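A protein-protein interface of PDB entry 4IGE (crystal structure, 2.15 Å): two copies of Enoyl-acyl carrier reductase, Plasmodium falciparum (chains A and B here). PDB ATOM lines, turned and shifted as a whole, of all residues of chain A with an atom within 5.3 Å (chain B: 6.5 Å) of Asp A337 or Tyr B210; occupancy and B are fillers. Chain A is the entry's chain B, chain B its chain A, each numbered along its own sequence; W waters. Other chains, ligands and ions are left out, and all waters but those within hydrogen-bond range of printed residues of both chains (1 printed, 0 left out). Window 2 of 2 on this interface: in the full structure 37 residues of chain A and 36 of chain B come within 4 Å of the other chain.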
ATOM      1  N   TYR A 292      -6.676   8.388 -26.867  1.00  0.00           N
ATOM      2  CA  TYR A 292      -6.905   9.555 -26.019  1.00  0.00           C
ATOM      3  C   TYR A 292      -5.843   9.842 -24.949  1.00  0.00           C
ATOM      4  O   TYR A 292      -5.843  10.929 -24.384  1.00  0.00           O
ATOM      5  CB  TYR A 292      -8.299   9.479 -25.360  1.00  0.00           C
ATOM      6  CG  TYR A 292      -9.415   9.552 -26.373  1.00  0.00           C
ATOM      7  CD1 TYR A 292      -9.551  10.666 -27.200  1.00  0.00           C
ATOM      8  CD2 TYR A 292     -10.327   8.511 -26.515  1.00  0.00           C
ATOM      9  CE1 TYR A 292     -10.574  10.745 -28.138  1.00  0.00           C
ATOM     10  CE2 TYR A 292     -11.357   8.578 -27.460  1.00  0.00           C
ATOM     11  CZ  TYR A 292     -11.465   9.696 -28.266  1.00  0.00           C
ATOM     12  OH  TYR A 292     -12.464   9.775 -29.201  1.00  0.00           O
ATOM     13  N   PRO A 294      -2.456  11.027 -23.103  1.00  0.00           N
ATOM     14  CA  PRO A 294      -1.363  11.969 -23.370  1.00  0.00           C
ATOM     15  C   PRO A 294      -0.255  11.311 -24.157  1.00  0.00           C
ATOM     16  O   PRO A 294       0.240  11.906 -25.101  1.00  0.00           O
ATOM     17  CB  PRO A 294      -0.883  12.333 -21.967  1.00  0.00           C
ATOM     18  CG  PRO A 294      -2.126  12.303 -21.168  1.00  0.00           C
ATOM     19  CD  PRO A 294      -2.880  11.097 -21.689  1.00  0.00           C
ATOM     20  N   ILE A 332      -5.591  11.090 -16.216  1.00  0.00           N
ATOM     21  CA  ILE A 332      -5.654  12.518 -15.946  1.00  0.00           C
ATOM     22  C   ILE A 332      -6.664  13.244 -16.833  1.00  0.00           C
ATOM     23  O   ILE A 332      -6.960  14.405 -16.582  1.00  0.00           O
ATOM     24  CB  ILE A 332      -4.275  13.230 -16.152  1.00  0.00           C
ATOM     25  CG1 ILE A 332      -3.987  13.459 -17.648  1.00  0.00           C
ATOM     26  CG2 ILE A 332      -3.171  12.475 -15.472  1.00  0.00           C
ATOM     27  CD1 ILE A 332      -2.631  14.099 -17.940  1.00  0.00           C
ATOM     28  N   MET A 333      -7.147  12.580 -17.882  1.00  0.00           N
ATOM     29  CA  MET A 333      -8.104  13.182 -18.817  1.00  0.00           C
ATOM     30  C   MET A 333      -9.538  13.211 -18.261  1.00  0.00           C
ATOM     31  O   MET A 333      -9.962  12.277 -17.568  1.00  0.00           O
ATOM     32  CB  MET A 333      -8.081  12.432 -20.157  1.00  0.00           C
ATOM     33  CG  MET A 333      -6.668  12.295 -20.753  1.00  0.00           C
ATOM     34  SD  MET A 333      -5.884  13.919 -21.004  1.00  0.00           S
ATOM     35  CE  MET A 333      -7.057  14.739 -22.101  1.00  0.00           C
ATOM     36  N   LEU A 335     -12.363  15.123 -20.409  1.00  0.00           N
ATOM     37  CA  LEU A 335     -13.056  15.122 -21.689  1.00  0.00           C
ATOM     38  C   LEU A 335     -12.126  14.699 -22.825  1.00  0.00           C
ATOM     39  O   LEU A 335     -11.089  15.326 -23.054  1.00  0.00           O
ATOM     40  CB  LEU A 335     -13.657  16.515 -21.983  1.00  0.00           C
ATOM     41  CG  LEU A 335     -14.712  17.043 -20.997  1.00  0.00           C
ATOM     42  CD1 LEU A 335     -15.273  18.395 -21.422  1.00  0.00           C
ATOM     43  CD2 LEU A 335     -15.847  16.040 -20.803  1.00  0.00           C
ATOM     44  N   PRO A 336     -12.499  13.628 -23.538  1.00  0.00           N
ATOM     45  CA  PRO A 336     -11.790  13.256 -24.766  1.00  0.00           C
ATOM     46  C   PRO A 336     -11.949  14.342 -25.821  1.00  0.00           C
ATOM     47  O   PRO A 336     -13.070  14.754 -26.103  1.00  0.00           O
ATOM     48  CB  PRO A 336     -12.510  11.981 -25.219  1.00  0.00           C
ATOM     49  CG  PRO A 336     -13.843  12.018 -24.547  1.00  0.00           C
ATOM     50  CD  PRO A 336     -13.612  12.712 -23.234  1.00  0.00           C
ATOM     51  N   ASP A 337     -10.836  14.806 -26.381  1.00  0.00           N
ATOM     52  CA  ASP A 337     -10.855  15.803 -27.449  1.00  0.00           C
ATOM     53  C   ASP A 337     -11.281  15.215 -28.796  1.00  0.00           C
ATOM     54  O   ASP A 337     -12.456  15.283 -29.176  1.00  0.00           O
ATOM     55  CB  ASP A 337      -9.482  16.476 -27.570  1.00  0.00           C
ATOM     56  CG  ASP A 337      -8.321  15.472 -27.579  1.00  0.00           C
ATOM     57  OD1 ASP A 337      -8.524  14.286 -27.232  1.00  0.00           O
ATOM     58  OD2 ASP A 337      -7.190  15.882 -27.921  1.00  0.00           O
ATOM     59  N   THR B 205       0.704  20.388 -14.023  1.00  0.00           N
ATOM     60  CA  THR B 205       1.462  19.194 -14.403  1.00  0.00           C
ATOM     61  C   THR B 205       0.601  18.272 -15.282  1.00  0.00           C
ATOM     62  O   THR B 205       1.075  17.765 -16.303  1.00  0.00           O
ATOM     63  CB  THR B 205       2.011  18.462 -13.147  1.00  0.00           C
ATOM     64  OG1 THR B 205       2.975  19.295 -12.495  1.00  0.00           O
ATOM     65  CG2 THR B 205       2.634  17.096 -13.472  1.00  0.00           C
ATOM     66  N   ARG B 206      -0.663  18.076 -14.908  1.00  0.00           N
ATOM     67  CA  ARG B 206      -1.575  17.310 -15.769  1.00  0.00           C
ATOM     68  C   ARG B 206      -1.810  17.971 -17.117  1.00  0.00           C
ATOM     69  O   ARG B 206      -1.784  17.306 -18.165  1.00  0.00           O
ATOM     70  CB  ARG B 206      -2.944  17.089 -15.095  1.00  0.00           C
ATOM     71  CG  ARG B 206      -2.871  16.218 -13.830  1.00  0.00           C
ATOM     72  CD  ARG B 206      -4.226  16.062 -13.198  1.00  0.00           C
ATOM     73  NE  ARG B 206      -4.647  17.243 -12.428  1.00  0.00           N
ATOM     74  CZ  ARG B 206      -4.433  17.409 -11.125  1.00  0.00           C
ATOM     75  NH1 ARG B 206      -3.763  16.486 -10.453  1.00  0.00           N
ATOM     76  NH2 ARG B 206      -4.865  18.502 -10.493  1.00  0.00           N
ATOM     77  N   VAL B 207      -2.101  19.267 -17.115  1.00  0.00           N
ATOM     78  CA  VAL B 207      -2.495  19.892 -18.379  1.00  0.00           C
ATOM     79  C   VAL B 207      -1.278  19.935 -19.318  1.00  0.00           C
ATOM     80  O   VAL B 207      -1.390  19.641 -20.501  1.00  0.00           O
ATOM     81  CB  VAL B 207      -3.115  21.299 -18.199  1.00  0.00           C
ATOM     82  CG1 VAL B 207      -3.308  21.964 -19.565  1.00  0.00           C
ATOM     83  CG2 VAL B 207      -4.466  21.231 -17.401  1.00  0.00           C
ATOM     84  N   LEU B 208      -0.117  20.266 -18.759  1.00  0.00           N
ATOM     85  CA  LEU B 208       1.141  20.220 -19.505  1.00  0.00           C
ATOM     86  C   LEU B 208       1.420  18.817 -20.019  1.00  0.00           C
ATOM     87  O   LEU B 208       1.885  18.654 -21.147  1.00  0.00           O
ATOM     88  CB  LEU B 208       2.308  20.696 -18.637  1.00  0.00           C
ATOM     89  CG  LEU B 208       2.264  22.210 -18.362  1.00  0.00           C
ATOM     90  CD1 LEU B 208       3.268  22.611 -17.287  1.00  0.00           C
ATOM     91  CD2 LEU B 208       2.536  22.955 -19.643  1.00  0.00           C
ATOM     92  N   ALA B 209       1.146  17.807 -19.189  1.00  0.00           N
ATOM     93  CA  ALA B 209       1.340  16.413 -19.601  1.00  0.00           C
ATOM     94  C   ALA B 209       0.538  16.070 -20.861  1.00  0.00           C
ATOM     95  O   ALA B 209       1.053  15.404 -21.791  1.00  0.00           O
ATOM     96  CB  ALA B 209       1.008  15.455 -18.471  1.00  0.00           C
ATOM     97  N   TYR B 210      -0.712  16.526 -20.891  1.00  0.00           N
ATOM     98  CA  TYR B 210      -1.518  16.422 -22.107  1.00  0.00           C
ATOM     99  C   TYR B 210      -0.856  17.078 -23.343  1.00  0.00           C
ATOM    100  O   TYR B 210      -0.671  16.410 -24.353  1.00  0.00           O
ATOM    101  CB  TYR B 210      -2.911  17.022 -21.891  1.00  0.00           C
ATOM    102  CG  TYR B 210      -3.744  17.104 -23.158  1.00  0.00           C
ATOM    103  CD1 TYR B 210      -4.330  15.972 -23.703  1.00  0.00           C
ATOM    104  CD2 TYR B 210      -3.944  18.323 -23.800  1.00  0.00           C
ATOM    105  CE1 TYR B 210      -5.107  16.041 -24.868  1.00  0.00           C
ATOM    106  CE2 TYR B 210      -4.698  18.411 -24.948  1.00  0.00           C
ATOM    107  CZ  TYR B 210      -5.280  17.273 -25.479  1.00  0.00           C
ATOM    108  OH  TYR B 210      -6.028  17.398 -26.620  1.00  0.00           O
ATOM    109  N   HIS B 211      -0.521  18.373 -23.264  1.00  0.00           N
ATOM    110  CA  HIS B 211       0.034  19.094 -24.414  1.00  0.00           C
ATOM    111  C   HIS B 211       1.426  18.582 -24.791  1.00  0.00           C
ATOM    112  O   HIS B 211       1.705  18.380 -25.966  1.00  0.00           O
ATOM    113  CB  HIS B 211       0.098  20.617 -24.175  1.00  0.00           C
ATOM    114  CG  HIS B 211      -1.229  21.258 -23.894  1.00  0.00           C
ATOM    115  ND1 HIS B 211      -2.239  21.331 -24.831  1.00  0.00           N
ATOM    116  CD2 HIS B 211      -1.697  21.887 -22.788  1.00  0.00           C
ATOM    117  CE1 HIS B 211      -3.280  21.953 -24.306  1.00  0.00           C
ATOM    118  NE2 HIS B 211      -2.978  22.300 -23.068  1.00  0.00           N
ATOM    119  N   LEU B 212       2.295  18.379 -23.801  1.00  0.00           N
ATOM    120  CA  LEU B 212       3.660  17.902 -24.071  1.00  0.00           C
ATOM    121  C   LEU B 212       3.638  16.473 -24.587  1.00  0.00           C
ATOM    122  O   LEU B 212       4.416  16.106 -25.485  1.00  0.00           O
ATOM    123  CB  LEU B 212       4.536  17.999 -22.818  1.00  0.00           C
ATOM    124  CG  LEU B 212       4.780  19.450 -22.387  1.00  0.00           C
ATOM    125  CD1 LEU B 212       5.579  19.508 -21.110  1.00  0.00           C
ATOM    126  CD2 LEU B 212       5.492  20.228 -23.496  1.00  0.00           C
ATOM    127  N   GLY B 213       2.723  15.674 -24.037  1.00  0.00           N
ATOM    128  CA  GLY B 213       2.631  14.274 -24.411  1.00  0.00           C
ATOM    129  C   GLY B 213       2.171  14.130 -25.849  1.00  0.00           C
ATOM    130  O   GLY B 213       2.822  13.473 -26.647  1.00  0.00           O
ATOM    131  N   ARG B 214       1.056  14.768 -26.186  1.00  0.00           N
ATOM    132  CA  ARG B 214       0.478  14.636 -27.525  1.00  0.00           C
ATOM    133  C   ARG B 214       1.317  15.315 -28.596  1.00  0.00           C
ATOM    134  O   ARG B 214       1.404  14.826 -29.709  1.00  0.00           O
ATOM    135  CB  ARG B 214      -0.925  15.244 -27.584  1.00  0.00           C
ATOM    136  CG  ARG B 214      -1.953  14.529 -26.766  1.00  0.00           C
ATOM    137  CD  ARG B 214      -2.335  13.210 -27.379  1.00  0.00           C
ATOM    138  NE  ARG B 214      -3.554  12.754 -26.732  1.00  0.00           N
ATOM    139  CZ  ARG B 214      -4.768  13.174 -27.081  1.00  0.00           C
ATOM    140  NH1 ARG B 214      -4.899  14.021 -28.096  1.00  0.00           N
ATOM    141  NH2 ARG B 214      -5.846  12.744 -26.426  1.00  0.00           N
ATOM    142  N   ASN B 215       1.905  16.456 -28.267  1.00  0.00           N
ATOM    143  CA  ASN B 215       2.610  17.236 -29.271  1.00  0.00           C
ATOM    144  C   ASN B 215       4.065  16.845 -29.431  1.00  0.00           C
ATOM    145  O   ASN B 215       4.559  16.847 -30.546  1.00  0.00           O
ATOM    146  CB  ASN B 215       2.475  18.743 -29.002  1.00  0.00           C
ATOM    147  CG  ASN B 215       1.069  19.252 -29.276  1.00  0.00           C
ATOM    148  OD1 ASN B 215       0.540  19.064 -30.372  1.00  0.00           O
ATOM    149  ND2 ASN B 215       0.444  19.868 -28.277  1.00  0.00           N
ATOM    150  N   ILE B 220       5.886  14.675 -18.210  1.00  0.00           N
ATOM    151  CA  ILE B 220       6.100  15.572 -17.095  1.00  0.00           C
ATOM    152  C   ILE B 220       5.353  15.065 -15.861  1.00  0.00           C
ATOM    153  O   ILE B 220       4.188  14.624 -15.960  1.00  0.00           O
ATOM    154  CB  ILE B 220       5.759  17.032 -17.473  1.00  0.00           C
ATOM    155  CG1 ILE B 220       6.034  17.973 -16.305  1.00  0.00           C
ATOM    156  CG2 ILE B 220       4.294  17.164 -17.955  1.00  0.00           C
ATOM    157  CD1 ILE B 220       5.645  19.413 -16.558  1.00  0.00           C
ATOM    158  N   THR B 320       3.036   9.711 -16.752  1.00  0.00           N
ATOM    159  CA  THR B 320       3.069  11.134 -17.037  1.00  0.00           C
ATOM    160  C   THR B 320       1.894  11.867 -16.405  1.00  0.00           C
ATOM    161  O   THR B 320       0.820  11.298 -16.212  1.00  0.00           O
ATOM    162  CB  THR B 320       3.187  11.408 -18.550  1.00  0.00           C
ATOM    163  OG1 THR B 320       3.456  12.792 -18.735  1.00  0.00           O
ATOM    164  CG2 THR B 320       1.930  11.044 -19.276  1.00  0.00           C
ATOM    165  N   GLY B 321       2.116  13.115 -16.015  1.00  0.00           N
ATOM    166  CA  GLY B 321       1.042  13.893 -15.439  1.00  0.00           C
ATOM    167  C   GLY B 321       0.764  13.548 -13.979  1.00  0.00           C
ATOM    168  O   GLY B 321      -0.250  13.963 -13.436  1.00  0.00           O
HETATM  169  O   HOH W   1       1.188  10.767 -27.510  1.00  0.00           O
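O of Ile B220 lies within hydrogen-bond range of N of Gly B321 (2.6 Å).
Printed residues of chain B within 4 Å of Pro A294: Ala B209, Gly B213 and Arg B214.
Printed residues of chain B within 4 Å of Ile A332: Arg B206 (3.3 Å), Ala B209 (3.9 Å) and Gly B321 (3.9 Å).
Of chain B, only Tyr B210 and Arg B214 come within 4 Å of Asp A337.
Printed residues of chain A within 4 Å of Ala B209: Pro A294 (3.6 Å) and Ile A332 (3.9 Å).
Of the printed residues of chain A, Tyr B210 touches Met A333 (3.4 Å) and Asp A337 (2.3 Å).
Ile B220 touches none of the printed residues of chain A.
Thr B320 touches none of the printed residues of chain A.
The nearest residue of chain A that does not touch Tyr B210 is Pro A294 (4.1 Å).
Water W1 bridges the backbone carbonyl oxygen (O) of Pro A294 (2.8 Å) and the backbone carbonyl oxygen (O) of Gly B213 (3.3 Å).
No position is printed for both chains.
O of Gly B213 sits close to O of Pro A294 (3.4 Å).
The side-chain carboxylate (OD2) of Asp A337 sits close to the side-chain hydroxyl (OH) of Tyr B210.
The guanidinium group of Arg B214 lies within salt-bridge range of the side-chain carboxylate of Asp A337, 3.0 Å away.
The backbone NH (N) of Arg B214 lies within hydrogen-bond range of the backbone carbonyl oxygen (O) of Pro A294 (3.2 Å).
NH2 of Arg B214 is in hydrogen-bond range of O of Tyr A292, at 2.7 Å.
Printed residues of chain B that touch a printed residue of chain A: Arg B206, Ala B209, Tyr B210, Gly B213, Arg B214 and Gly B321.
Hydrophobic or aromatic side chains of chain B that line the printed part of chain A: Ala B209 and Tyr B210.
Printed residues of chain A that touch a printed residue of chain B: Tyr A292, Pro A294, Ile A332, Met A333 and Asp A337.
Among the printed residues, 10 pairs touch across the chains.
Among the printed residues, Asp or Glu carboxylates within 4 Å of a Lys or Arg side-chain nitrogen of the other chain: Asp A337 with Arg B214.
CB of Pro A294 touches O of Ala B209, at 3.6 Å.
CD1 of Ile A332 touches O of Arg B206 (3.3 Å).
Ile A332 touches Ala B209 (CD1 to CB, 3.9 Å).
Gly B321 touches Ile A332.
Met A333 touches Tyr B210.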
